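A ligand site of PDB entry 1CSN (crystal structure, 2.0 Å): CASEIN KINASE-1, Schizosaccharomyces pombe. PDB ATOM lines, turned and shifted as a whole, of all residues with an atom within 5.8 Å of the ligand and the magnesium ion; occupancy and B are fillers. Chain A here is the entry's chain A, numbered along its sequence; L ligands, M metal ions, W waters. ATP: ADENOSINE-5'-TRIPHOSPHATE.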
ATOM      1  N   ILE A  18       8.050 -17.688   5.154  1.00  0.00           N
ATOM      2  CA  ILE A  18       7.641 -18.644   6.190  1.00  0.00           C
ATOM      3  C   ILE A  18       7.649 -17.971   7.553  1.00  0.00           C
ATOM      4  O   ILE A  18       7.061 -18.477   8.509  1.00  0.00           O
ATOM      5  CB  ILE A  18       8.557 -19.878   6.237  1.00  0.00           C
ATOM      6  CG1 ILE A  18      10.008 -19.454   6.450  1.00  0.00           C
ATOM      7  CG2 ILE A  18       8.396 -20.688   4.965  1.00  0.00           C
ATOM      8  CD1 ILE A  18      10.954 -20.613   6.656  1.00  0.00           C
ATOM      9  N   GLY A  19       8.296 -16.820   7.654  1.00  0.00           N
ATOM     10  CA  GLY A  19       8.355 -16.125   8.912  1.00  0.00           C
ATOM     11  C   GLY A  19       8.695 -14.656   8.732  1.00  0.00           C
ATOM     12  O   GLY A  19       9.215 -14.234   7.690  1.00  0.00           O
ATOM     13  N   GLU A  20       8.409 -13.882   9.770  1.00  0.00           N
ATOM     14  CA  GLU A  20       8.657 -12.459   9.758  1.00  0.00           C
ATOM     15  C   GLU A  20       9.057 -12.071  11.184  1.00  0.00           C
ATOM     16  O   GLU A  20       8.633 -12.704  12.155  1.00  0.00           O
ATOM     17  CB  GLU A  20       7.375 -11.735   9.354  1.00  0.00           C
ATOM     18  CG  GLU A  20       7.582 -10.348   8.752  1.00  0.00           C
ATOM     19  CD  GLU A  20       6.290  -9.736   8.227  1.00  0.00           C
ATOM     20  OE1 GLU A  20       5.203 -10.285   8.523  1.00  0.00           O
ATOM     21  OE2 GLU A  20       6.356  -8.716   7.513  1.00  0.00           O
ATOM     22  N   GLY A  21       9.941 -11.092  11.303  1.00  0.00           N
ATOM     23  CA  GLY A  21      10.380 -10.651  12.607  1.00  0.00           C
ATOM     24  C   GLY A  21      10.253  -9.146  12.687  1.00  0.00           C
ATOM     25  O   GLY A  21       9.457  -8.553  11.969  1.00  0.00           O
ATOM     26  N   SER A  22      11.056  -8.529  13.551  1.00  0.00           N
ATOM     27  CA  SER A  22      11.029  -7.079  13.713  1.00  0.00           C
ATOM     28  C   SER A  22      11.510  -6.367  12.447  1.00  0.00           C
ATOM     29  O   SER A  22      10.873  -5.416  11.981  1.00  0.00           O
ATOM     30  CB  SER A  22      11.871  -6.660  14.911  1.00  0.00           C
ATOM     31  OG  SER A  22      11.383  -7.272  16.099  1.00  0.00           O
ATOM     32  N   PHE A  23      12.635  -6.820  11.894  1.00  0.00           N
ATOM     33  CA  PHE A  23      13.199  -6.224  10.680  1.00  0.00           C
ATOM     34  C   PHE A  23      13.411  -7.224   9.535  1.00  0.00           C
ATOM     35  O   PHE A  23      13.490  -6.818   8.369  1.00  0.00           O
ATOM     36  CB  PHE A  23      14.539  -5.552  10.987  1.00  0.00           C
ATOM     37  CG  PHE A  23      14.445  -4.338  11.864  1.00  0.00           C
ATOM     38  CD1 PHE A  23      14.210  -3.081  11.308  1.00  0.00           C
ATOM     39  CD2 PHE A  23      14.593  -4.446  13.245  1.00  0.00           C
ATOM     40  CE1 PHE A  23      14.127  -1.954  12.112  1.00  0.00           C
ATOM     41  CE2 PHE A  23      14.511  -3.318  14.059  1.00  0.00           C
ATOM     42  CZ  PHE A  23      14.276  -2.062  13.493  1.00  0.00           C
ATOM     43  N   GLY A  24      13.509  -8.506   9.871  1.00  0.00           N
ATOM     44  CA  GLY A  24      13.754  -9.503   8.853  1.00  0.00           C
ATOM     45  C   GLY A  24      12.599 -10.377   8.418  1.00  0.00           C
ATOM     46  O   GLY A  24      11.622 -10.570   9.140  1.00  0.00           O
ATOM     47  N   VAL A  25      12.749 -10.927   7.214  1.00  0.00           N
ATOM     48  CA  VAL A  25      11.769 -11.829   6.612  1.00  0.00           C
ATOM     49  C   VAL A  25      12.527 -13.120   6.330  1.00  0.00           C
ATOM     50  O   VAL A  25      13.679 -13.092   5.882  1.00  0.00           O
ATOM     51  CB  VAL A  25      11.208 -11.271   5.272  1.00  0.00           C
ATOM     52  CG1 VAL A  25      10.078 -12.168   4.754  1.00  0.00           C
ATOM     53  CG2 VAL A  25      10.708  -9.847   5.453  1.00  0.00           C
ATOM     54  N   ILE A  26      11.906 -14.247   6.649  1.00  0.00           N
ATOM     55  CA  ILE A  26      12.528 -15.536   6.439  1.00  0.00           C
ATOM     56  C   ILE A  26      11.763 -16.272   5.350  1.00  0.00           C
ATOM     57  O   ILE A  26      10.519 -16.337   5.374  1.00  0.00           O
ATOM     58  CB  ILE A  26      12.587 -16.381   7.768  1.00  0.00           C
ATOM     59  CG1 ILE A  26      13.587 -15.760   8.755  1.00  0.00           C
ATOM     60  CG2 ILE A  26      13.073 -17.795   7.488  1.00  0.00           C
ATOM     61  CD1 ILE A  26      13.106 -14.540   9.464  1.00  0.00           C
ATOM     62  N   ALA A  39      16.523 -22.189   4.850  1.00  0.00           N
ATOM     63  CA  ALA A  39      15.758 -21.026   5.241  1.00  0.00           C
ATOM     64  C   ALA A  39      16.712 -19.876   5.014  1.00  0.00           C
ATOM     65  O   ALA A  39      17.896 -19.961   5.345  1.00  0.00           O
ATOM     66  CB  ALA A  39      15.345 -21.106   6.700  1.00  0.00           C
ATOM     67  N   LYS A  41      17.253 -15.848   5.704  1.00  0.00           N
ATOM     68  CA  LYS A  41      16.864 -14.704   6.505  1.00  0.00           C
ATOM     69  C   LYS A  41      17.390 -13.435   5.865  1.00  0.00           C
ATOM     70  O   LYS A  41      18.602 -13.280   5.684  1.00  0.00           O
ATOM     71  CB  LYS A  41      17.417 -14.869   7.931  1.00  0.00           C
ATOM     72  CG  LYS A  41      17.004 -13.758   8.904  1.00  0.00           C
ATOM     73  CD  LYS A  41      17.451 -14.081  10.327  1.00  0.00           C
ATOM     74  CE  LYS A  41      16.874 -13.099  11.342  1.00  0.00           C
ATOM     75  NZ  LYS A  41      17.167 -13.503  12.748  1.00  0.00           N
ATOM     76  N   GLU A  43      17.762  -9.420   6.026  1.00  0.00           N
ATOM     77  CA  GLU A  43      17.837  -8.349   6.997  1.00  0.00           C
ATOM     78  C   GLU A  43      18.240  -7.058   6.318  1.00  0.00           C
ATOM     79  O   GLU A  43      19.272  -6.993   5.669  1.00  0.00           O
ATOM     80  CB  GLU A  43      18.862  -8.679   8.081  1.00  0.00           C
ATOM     81  CG  GLU A  43      18.369  -9.640   9.154  1.00  0.00           C
ATOM     82  CD  GLU A  43      18.113  -8.941  10.479  1.00  0.00           C
ATOM     83  OE1 GLU A  43      18.760  -7.904  10.759  1.00  0.00           O
ATOM     84  OE2 GLU A  43      17.266  -9.443  11.257  1.00  0.00           O
ATOM     85  N   PRO A  50      19.470  -5.264  13.674  1.00  0.00           N
ATOM     86  CA  PRO A  50      20.517  -6.109  14.257  1.00  0.00           C
ATOM     87  C   PRO A  50      21.483  -6.619  13.185  1.00  0.00           C
ATOM     88  O   PRO A  50      21.053  -7.111  12.141  1.00  0.00           O
ATOM     89  CB  PRO A  50      19.713  -7.250  14.882  1.00  0.00           C
ATOM     90  CG  PRO A  50      18.561  -7.395  13.934  1.00  0.00           C
ATOM     91  CD  PRO A  50      18.166  -5.970  13.665  1.00  0.00           C
ATOM     92  N   GLU A  55      25.115 -12.620  14.064  1.00  0.00           N
ATOM     93  CA  GLU A  55      24.344 -13.849  14.203  1.00  0.00           C
ATOM     94  C   GLU A  55      25.077 -14.972  13.464  1.00  0.00           C
ATOM     95  O   GLU A  55      25.061 -16.133  13.882  1.00  0.00           O
ATOM     96  CB  GLU A  55      22.946 -13.658  13.642  1.00  0.00           C
ATOM     97  CG  GLU A  55      22.098 -14.906  13.737  1.00  0.00           C
ATOM     98  CD  GLU A  55      20.613 -14.621  13.686  1.00  0.00           C
ATOM     99  OE1 GLU A  55      20.194 -13.499  13.345  1.00  0.00           O
ATOM    100  OE2 GLU A  55      19.845 -15.545  14.000  1.00  0.00           O
ATOM    101  N   PRO A  69      20.862 -25.172  14.450  1.00  0.00           N
ATOM    102  CA  PRO A  69      20.904 -25.380  12.998  1.00  0.00           C
ATOM    103  C   PRO A  69      22.255 -25.006  12.357  1.00  0.00           C
ATOM    104  O   PRO A  69      23.004 -24.189  12.896  1.00  0.00           O
ATOM    105  CB  PRO A  69      19.764 -24.474  12.484  1.00  0.00           C
ATOM    106  CG  PRO A  69      19.675 -23.397  13.530  1.00  0.00           C
ATOM    107  CD  PRO A  69      19.831 -24.175  14.811  1.00  0.00           C
ATOM    108  N   ILE A  85      20.433 -20.901   6.523  1.00  0.00           N
ATOM    109  CA  ILE A  85      20.573 -21.890   7.582  1.00  0.00           C
ATOM    110  C   ILE A  85      19.611 -23.016   7.267  1.00  0.00           C
ATOM    111  O   ILE A  85      18.870 -22.943   6.287  1.00  0.00           O
ATOM    112  CB  ILE A  85      20.208 -21.307   8.975  1.00  0.00           C
ATOM    113  CG1 ILE A  85      18.760 -20.819   8.984  1.00  0.00           C
ATOM    114  CG2 ILE A  85      21.151 -20.150   9.362  1.00  0.00           C
ATOM    115  CD1 ILE A  85      18.309 -20.246  10.294  1.00  0.00           C
ATOM    116  N   ASP A  86      19.622 -24.060   8.076  1.00  0.00           N
ATOM    117  CA  ASP A  86      18.726 -25.180   7.856  1.00  0.00           C
ATOM    118  C   ASP A  86      17.262 -24.791   7.975  1.00  0.00           C
ATOM    119  O   ASP A  86      16.902 -23.928   8.779  1.00  0.00           O
ATOM    120  CB  ASP A  86      18.998 -26.314   8.832  1.00  0.00           C
ATOM    121  CG  ASP A  86      20.244 -27.082   8.475  1.00  0.00           C
ATOM    122  OD1 ASP A  86      20.354 -27.514   7.306  1.00  0.00           O
ATOM    123  OD2 ASP A  86      21.093 -27.255   9.365  1.00  0.00           O
ATOM    124  N   LEU A  87      16.430 -25.462   7.183  1.00  0.00           N
ATOM    125  CA  LEU A  87      15.004 -25.226   7.227  1.00  0.00           C
ATOM    126  C   LEU A  87      14.447 -26.064   8.367  1.00  0.00           C
ATOM    127  O   LEU A  87      14.680 -27.269   8.412  1.00  0.00           O
ATOM    128  CB  LEU A  87      14.336 -25.667   5.922  1.00  0.00           C
ATOM    129  CG  LEU A  87      12.833 -25.400   5.933  1.00  0.00           C
ATOM    130  CD1 LEU A  87      12.561 -23.898   5.915  1.00  0.00           C
ATOM    131  CD2 LEU A  87      12.182 -26.078   4.764  1.00  0.00           C
ATOM    132  N   LEU A  88      13.741 -25.430   9.288  1.00  0.00           N
ATOM    133  CA  LEU A  88      13.171 -26.138  10.421  1.00  0.00           C
ATOM    134  C   LEU A  88      11.655 -26.105  10.379  1.00  0.00           C
ATOM    135  O   LEU A  88      11.074 -25.581   9.431  1.00  0.00           O
ATOM    136  CB  LEU A  88      13.694 -25.544  11.729  1.00  0.00           C
ATOM    137  CG  LEU A  88      15.209 -25.727  11.900  1.00  0.00           C
ATOM    138  CD1 LEU A  88      15.732 -24.919  13.061  1.00  0.00           C
ATOM    139  CD2 LEU A  88      15.508 -27.197  12.106  1.00  0.00           C
ATOM    140  N   GLY A  89      11.022 -26.712  11.388  1.00  0.00           N
ATOM    141  CA  GLY A  89       9.571 -26.752  11.450  1.00  0.00           C
ATOM    142  C   GLY A  89       8.960 -25.573  12.200  1.00  0.00           C
ATOM    143  O   GLY A  89       9.598 -24.520  12.350  1.00  0.00           O
ATOM    144  N   SER A  91       7.358 -23.207  15.317  1.00  0.00           N
ATOM    145  CA  SER A  91       7.841 -22.836  16.646  1.00  0.00           C
ATOM    146  C   SER A  91       6.872 -23.401  17.674  1.00  0.00           C
ATOM    147  O   SER A  91       5.758 -23.831  17.321  1.00  0.00           O
ATOM    148  CB  SER A  91       7.909 -21.313  16.811  1.00  0.00           C
ATOM    149  OG  SER A  91       6.611 -20.751  16.868  1.00  0.00           O
ATOM    150  N   ASP A  94       3.634 -21.571  17.621  1.00  0.00           N
ATOM    151  CA  ASP A  94       2.721 -22.031  16.568  1.00  0.00           C
ATOM    152  C   ASP A  94       2.008 -23.290  17.013  1.00  0.00           C
ATOM    153  O   ASP A  94       0.818 -23.482  16.760  1.00  0.00           O
ATOM    154  CB  ASP A  94       3.467 -22.378  15.276  1.00  0.00           C
ATOM    155  CG  ASP A  94       4.176 -21.196  14.659  1.00  0.00           C
ATOM    156  OD1 ASP A  94       3.721 -20.042  14.843  1.00  0.00           O
ATOM    157  OD2 ASP A  94       5.191 -21.421  13.978  1.00  0.00           O
ATOM    158  N   ASP A 131      17.097 -13.688  24.725  1.00  0.00           N
ATOM    159  CA  ASP A 131      15.856 -13.488  23.979  1.00  0.00           C
ATOM    160  C   ASP A 131      14.947 -14.708  24.080  1.00  0.00           C
ATOM    161  O   ASP A 131      14.345 -15.136  23.112  1.00  0.00           O
ATOM    162  CB  ASP A 131      16.152 -13.130  22.504  1.00  0.00           C
ATOM    163  CG  ASP A 131      14.946 -12.500  21.781  1.00  0.00           C
ATOM    164  OD1 ASP A 131      14.155 -11.768  22.409  1.00  0.00           O
ATOM    165  OD2 ASP A 131      14.804 -12.728  20.555  1.00  0.00           O
ATOM    166  N   LYS A 133      11.967 -16.908  24.304  1.00  0.00           N
ATOM    167  CA  LYS A 133      10.547 -16.815  23.963  1.00  0.00           C
ATOM    168  C   LYS A 133      10.201 -18.059  23.163  1.00  0.00           C
ATOM    169  O   LYS A 133      11.062 -18.593  22.471  1.00  0.00           O
ATOM    170  CB  LYS A 133      10.230 -15.540  23.174  1.00  0.00           C
ATOM    171  CG  LYS A 133      11.043 -15.318  21.914  1.00  0.00           C
ATOM    172  CD  LYS A 133      10.537 -14.070  21.200  1.00  0.00           C
ATOM    173  CE  LYS A 133      11.610 -13.497  20.284  1.00  0.00           C
ATOM    174  NZ  LYS A 133      11.201 -12.239  19.612  1.00  0.00           N
ATOM    175  N   ASP A 135       8.719 -18.452  20.483  1.00  0.00           N
ATOM    176  CA  ASP A 135       8.870 -18.210  19.059  1.00  0.00           C
ATOM    177  C   ASP A 135      10.227 -18.600  18.527  1.00  0.00           C
ATOM    178  O   ASP A 135      10.376 -18.872  17.337  1.00  0.00           O
ATOM    179  CB  ASP A 135       8.635 -16.733  18.757  1.00  0.00           C
ATOM    180  CG  ASP A 135       7.333 -16.216  19.335  1.00  0.00           C
ATOM    181  OD1 ASP A 135       7.314 -15.881  20.536  1.00  0.00           O
ATOM    182  OD2 ASP A 135       6.332 -16.160  18.588  1.00  0.00           O
ATOM    183  N   ASN A 136      11.232 -18.599  19.396  1.00  0.00           N
ATOM    184  CA  ASN A 136      12.592 -18.932  18.985  1.00  0.00           C
ATOM    185  C   ASN A 136      12.982 -20.393  19.154  1.00  0.00           C
ATOM    186  O   ASN A 136      14.118 -20.762  18.922  1.00  0.00           O
ATOM    187  CB  ASN A 136      13.597 -18.020  19.695  1.00  0.00           C
ATOM    188  CG  ASN A 136      13.496 -16.566  19.241  1.00  0.00           C
ATOM    189  OD1 ASN A 136      12.629 -16.199  18.436  1.00  0.00           O
ATOM    190  ND2 ASN A 136      14.408 -15.734  19.727  1.00  0.00           N
ATOM    191  N   LEU A 138      12.023 -24.018  17.762  1.00  0.00           N
ATOM    192  CA  LEU A 138      11.315 -24.696  16.669  1.00  0.00           C
ATOM    193  C   LEU A 138      11.577 -26.189  16.647  1.00  0.00           C
ATOM    194  O   LEU A 138      12.632 -26.636  17.084  1.00  0.00           O
ATOM    195  CB  LEU A 138      11.762 -24.128  15.304  1.00  0.00           C
ATOM    196  CG  LEU A 138      12.199 -22.672  15.115  1.00  0.00           C
ATOM    197  CD1 LEU A 138      12.475 -22.432  13.650  1.00  0.00           C
ATOM    198  CD2 LEU A 138      11.129 -21.712  15.580  1.00  0.00           C
ATOM    199  N   VAL A 153      16.796 -20.922  17.369  1.00  0.00           N
ATOM    200  CA  VAL A 153      17.217 -20.053  16.271  1.00  0.00           C
ATOM    201  C   VAL A 153      17.242 -18.618  16.799  1.00  0.00           C
ATOM    202  O   VAL A 153      16.914 -18.380  17.964  1.00  0.00           O
ATOM    203  CB  VAL A 153      16.250 -20.136  15.047  1.00  0.00           C
ATOM    204  CG1 VAL A 153      16.173 -21.550  14.533  1.00  0.00           C
ATOM    205  CG2 VAL A 153      14.867 -19.614  15.411  1.00  0.00           C
ATOM    206  N   ASP A 154      17.658 -17.684  15.953  1.00  0.00           N
ATOM    207  CA  ASP A 154      17.701 -16.273  16.319  1.00  0.00           C
ATOM    208  C   ASP A 154      18.677 -15.949  17.466  1.00  0.00           C
ATOM    209  O   ASP A 154      18.318 -15.914  18.641  1.00  0.00           O
ATOM    210  CB  ASP A 154      16.273 -15.781  16.627  1.00  0.00           C
ATOM    211  CG  ASP A 154      16.156 -14.270  16.737  1.00  0.00           C
ATOM    212  OD1 ASP A 154      17.177 -13.542  16.570  1.00  0.00           O
ATOM    213  OD2 ASP A 154      15.036 -13.803  16.999  1.00  0.00           O
HETATM  214  PG  ATP L   1      12.250 -11.178  15.974  1.00  0.00           P
HETATM  215  O1G ATP L   1      12.564 -12.161  17.059  1.00  0.00           O
HETATM  216  O2G ATP L   1      13.005  -9.919  15.937  1.00  0.00           O
HETATM  217  O3G ATP L   1      10.791 -11.159  15.697  1.00  0.00           O
HETATM  218  PB  ATP L   1      13.824 -11.804  13.484  1.00  0.00           P
HETATM  219  O1B ATP L   1      13.469 -10.596  12.677  1.00  0.00           O
HETATM  220  O2B ATP L   1      15.195 -11.948  13.999  1.00  0.00           O
HETATM  221  O3B ATP L   1      12.717 -12.046  14.689  1.00  0.00           O
HETATM  222  PA  ATP L   1      13.643 -14.596  13.363  1.00  0.00           P
HETATM  223  O1A ATP L   1      15.007 -15.022  13.041  1.00  0.00           O
HETATM  224  O2A ATP L   1      13.185 -14.670  14.796  1.00  0.00           O
HETATM  225  O3A ATP L   1      13.342 -13.160  12.765  1.00  0.00           O
HETATM  226  O5' ATP L   1      12.556 -15.470  12.640  1.00  0.00           O
HETATM  227  C5' ATP L   1      11.171 -15.190  12.681  1.00  0.00           C
HETATM  228  C4' ATP L   1      10.317 -16.443  12.466  1.00  0.00           C
HETATM  229  O4' ATP L   1      10.614 -17.197  11.286  1.00  0.00           O
HETATM  230  C3' ATP L   1      10.652 -17.422  13.539  1.00  0.00           C
HETATM  231  O3' ATP L   1      10.074 -16.939  14.768  1.00  0.00           O
HETATM  232  C2' ATP L   1       9.997 -18.671  12.975  1.00  0.00           C
HETATM  233  O2' ATP L   1       8.585 -18.494  12.937  1.00  0.00           O
HETATM  234  C1' ATP L   1      10.523 -18.619  11.537  1.00  0.00           C
HETATM  235  N9  ATP L   1      11.889 -19.217  11.333  1.00  0.00           N
HETATM  236  C8  ATP L   1      13.125 -18.660  11.577  1.00  0.00           C
HETATM  237  N7  ATP L   1      14.140 -19.392  11.230  1.00  0.00           N
HETATM  238  C5  ATP L   1      13.554 -20.528  10.723  1.00  0.00           C
HETATM  239  C6  ATP L   1      14.109 -21.680  10.199  1.00  0.00           C
HETATM  240  N6  ATP L   1      15.417 -21.886  10.246  1.00  0.00           N
HETATM  241  N1  ATP L   1      13.245 -22.632   9.768  1.00  0.00           N
HETATM  242  C2  ATP L   1      11.939 -22.448   9.871  1.00  0.00           C
HETATM  243  N3  ATP L   1      11.327 -21.389  10.358  1.00  0.00           N
HETATM  244  C4  ATP L   1      12.194 -20.458  10.779  1.00  0.00           C
HETATM  245 MG    MG M   1      11.743 -14.288  16.679  1.00  0.00          MG
HETATM  246  O   HOH W   1       6.527 -18.343  15.391  1.00  0.00           O
HETATM  247  O   HOH W   2       6.079 -17.927  11.500  1.00  0.00           O
HETATM  248  O   HOH W   3       8.959 -22.164  11.392  1.00  0.00           O
HETATM  249  O   HOH W   4       7.197 -20.543  12.576  1.00  0.00           O
HETATM  250  O   HOH W   5      16.144 -17.435  11.889  1.00  0.00           O
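Residues that only touch the magnesium ion: Asp 154 and Lys 133. Along chain A the residues within 4 Å of the magnesium ion span positions 133 to 154. The nearest printed residue that does not touch the magnesium ion is Asp 135 (4.5 Å).
O1B of the ligand is in hydrogen-bond range of N of Gly 24, 3.5 Å away. The backbone NH (N) of Leu 88 sits at hydrogen-bond distance from a nitrogen (N1) of the ligand, at 2.9 Å. O of Asp 86 lies within hydrogen-bond range of N6 of the ligand (2.9 Å). The side-chain amino group (NZ) of Lys 133 sits close to an oxygen (O1G) of the ligand (2.9 Å). An oxygen (O1A) of the ligand lies within salt-bridge range of the side-chain amino group (NZ) of Lys 41. The backbone NH (N) of Ser 22 lies within hydrogen-bond range of an oxygen (O1B) of the ligand (3.3 Å). OG of Ser 22 lies within hydrogen-bond range of O2G of the ligand (3.1 Å). The backbone carbonyl oxygen (O) of Asp 135 lies within hydrogen-bond range of an oxygen (O3') of the ligand, 3.2 Å away.
Water W4 lies within hydrogen-bond range of an oxygen (O2') of the ligand (2.5 Å) and the side-chain carboxylate (OD2) of Asp 94 (2.6 Å). Water W3 lies within hydrogen-bond range of O of Gly 89 (2.6 Å) and N3 of the ligand (2.7 Å). Water W2 bridges O2' of the ligand (2.9 Å) and O of Ile 18 (3.2 Å). Water W1 lies within hydrogen-bond range of OG of Ser 91 (2.8 Å), O2' of the ligand (3.2 Å) and OD1 of Asp 94 (3.3 Å).
The backbone NH (N) of Ile 18 sits at hydrogen-bond distance from the backbone carbonyl oxygen (O) of Ile 26 (2.8 Å). The side-chain carboxylate of Asp 131 is in salt-bridge range of the side-chain amino group of Lys 133 (3.8 Å). The backbone carbonyl oxygen of Gly 19 is in hydrogen-bond range of the backbone NH of Ile 26 (2.9 Å). O of Ile 85 lies within hydrogen-bond range of N of Ala 39, at 2.9 Å. The side-chain amino group (NZ) of Lys 41 lies within salt-bridge range of the side-chain carboxylate (OE1) of Glu 55. The side-chain amino group (NZ) of Lys 41 is in salt-bridge range of the side-chain carboxylate (OD1) of Asp 154, at 3.8 Å. The side-chain amide nitrogen (ND2) of Asn 136 lies within hydrogen-bond range of the side-chain carboxylate (OD2) of Asp 154 (3.4 Å). The backbone NH (N) of Val 153 is in hydrogen-bond range of the backbone carbonyl oxygen (O) of Asn 136.
The side-chain carboxylate of Asp 154 lies close to an oxygen (O1G) of the ligand, at 3.0 Å. Ile 18 touches the ligand (CD1 to N3, 3.8 Å). CA of Gly 19 touches O4' of the ligand, 3.4 Å away. Glu 20 touches the ligand (O to C5', 3.6 Å). CA of Gly 21 touches O1B of the ligand (3.1 Å). Phe 23 touches the ligand (N to O1B, 3.9 Å). Ile 26 touches the ligand (CD1 to O5', 3.4 Å). CB of Ala 39 touches N6 of the ligand, at 3.6 Å. Ile 85 touches the ligand. C of Leu 87 touches N1 of the ligand, at 3.9 Å. Gly 89 touches the ligand. Leu 138 touches the ligand.
The magnesium ion is bound by an oxygen (O1G) of the ligand (2.3 Å) and an oxygen (O2A) of the ligand (2.4 Å). The magnesium ion has two donor atoms within binding distance. Slightly farther from the magnesium ion lies the side-chain amide oxygen (OD1) of Asn 136 (2.7 Å).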
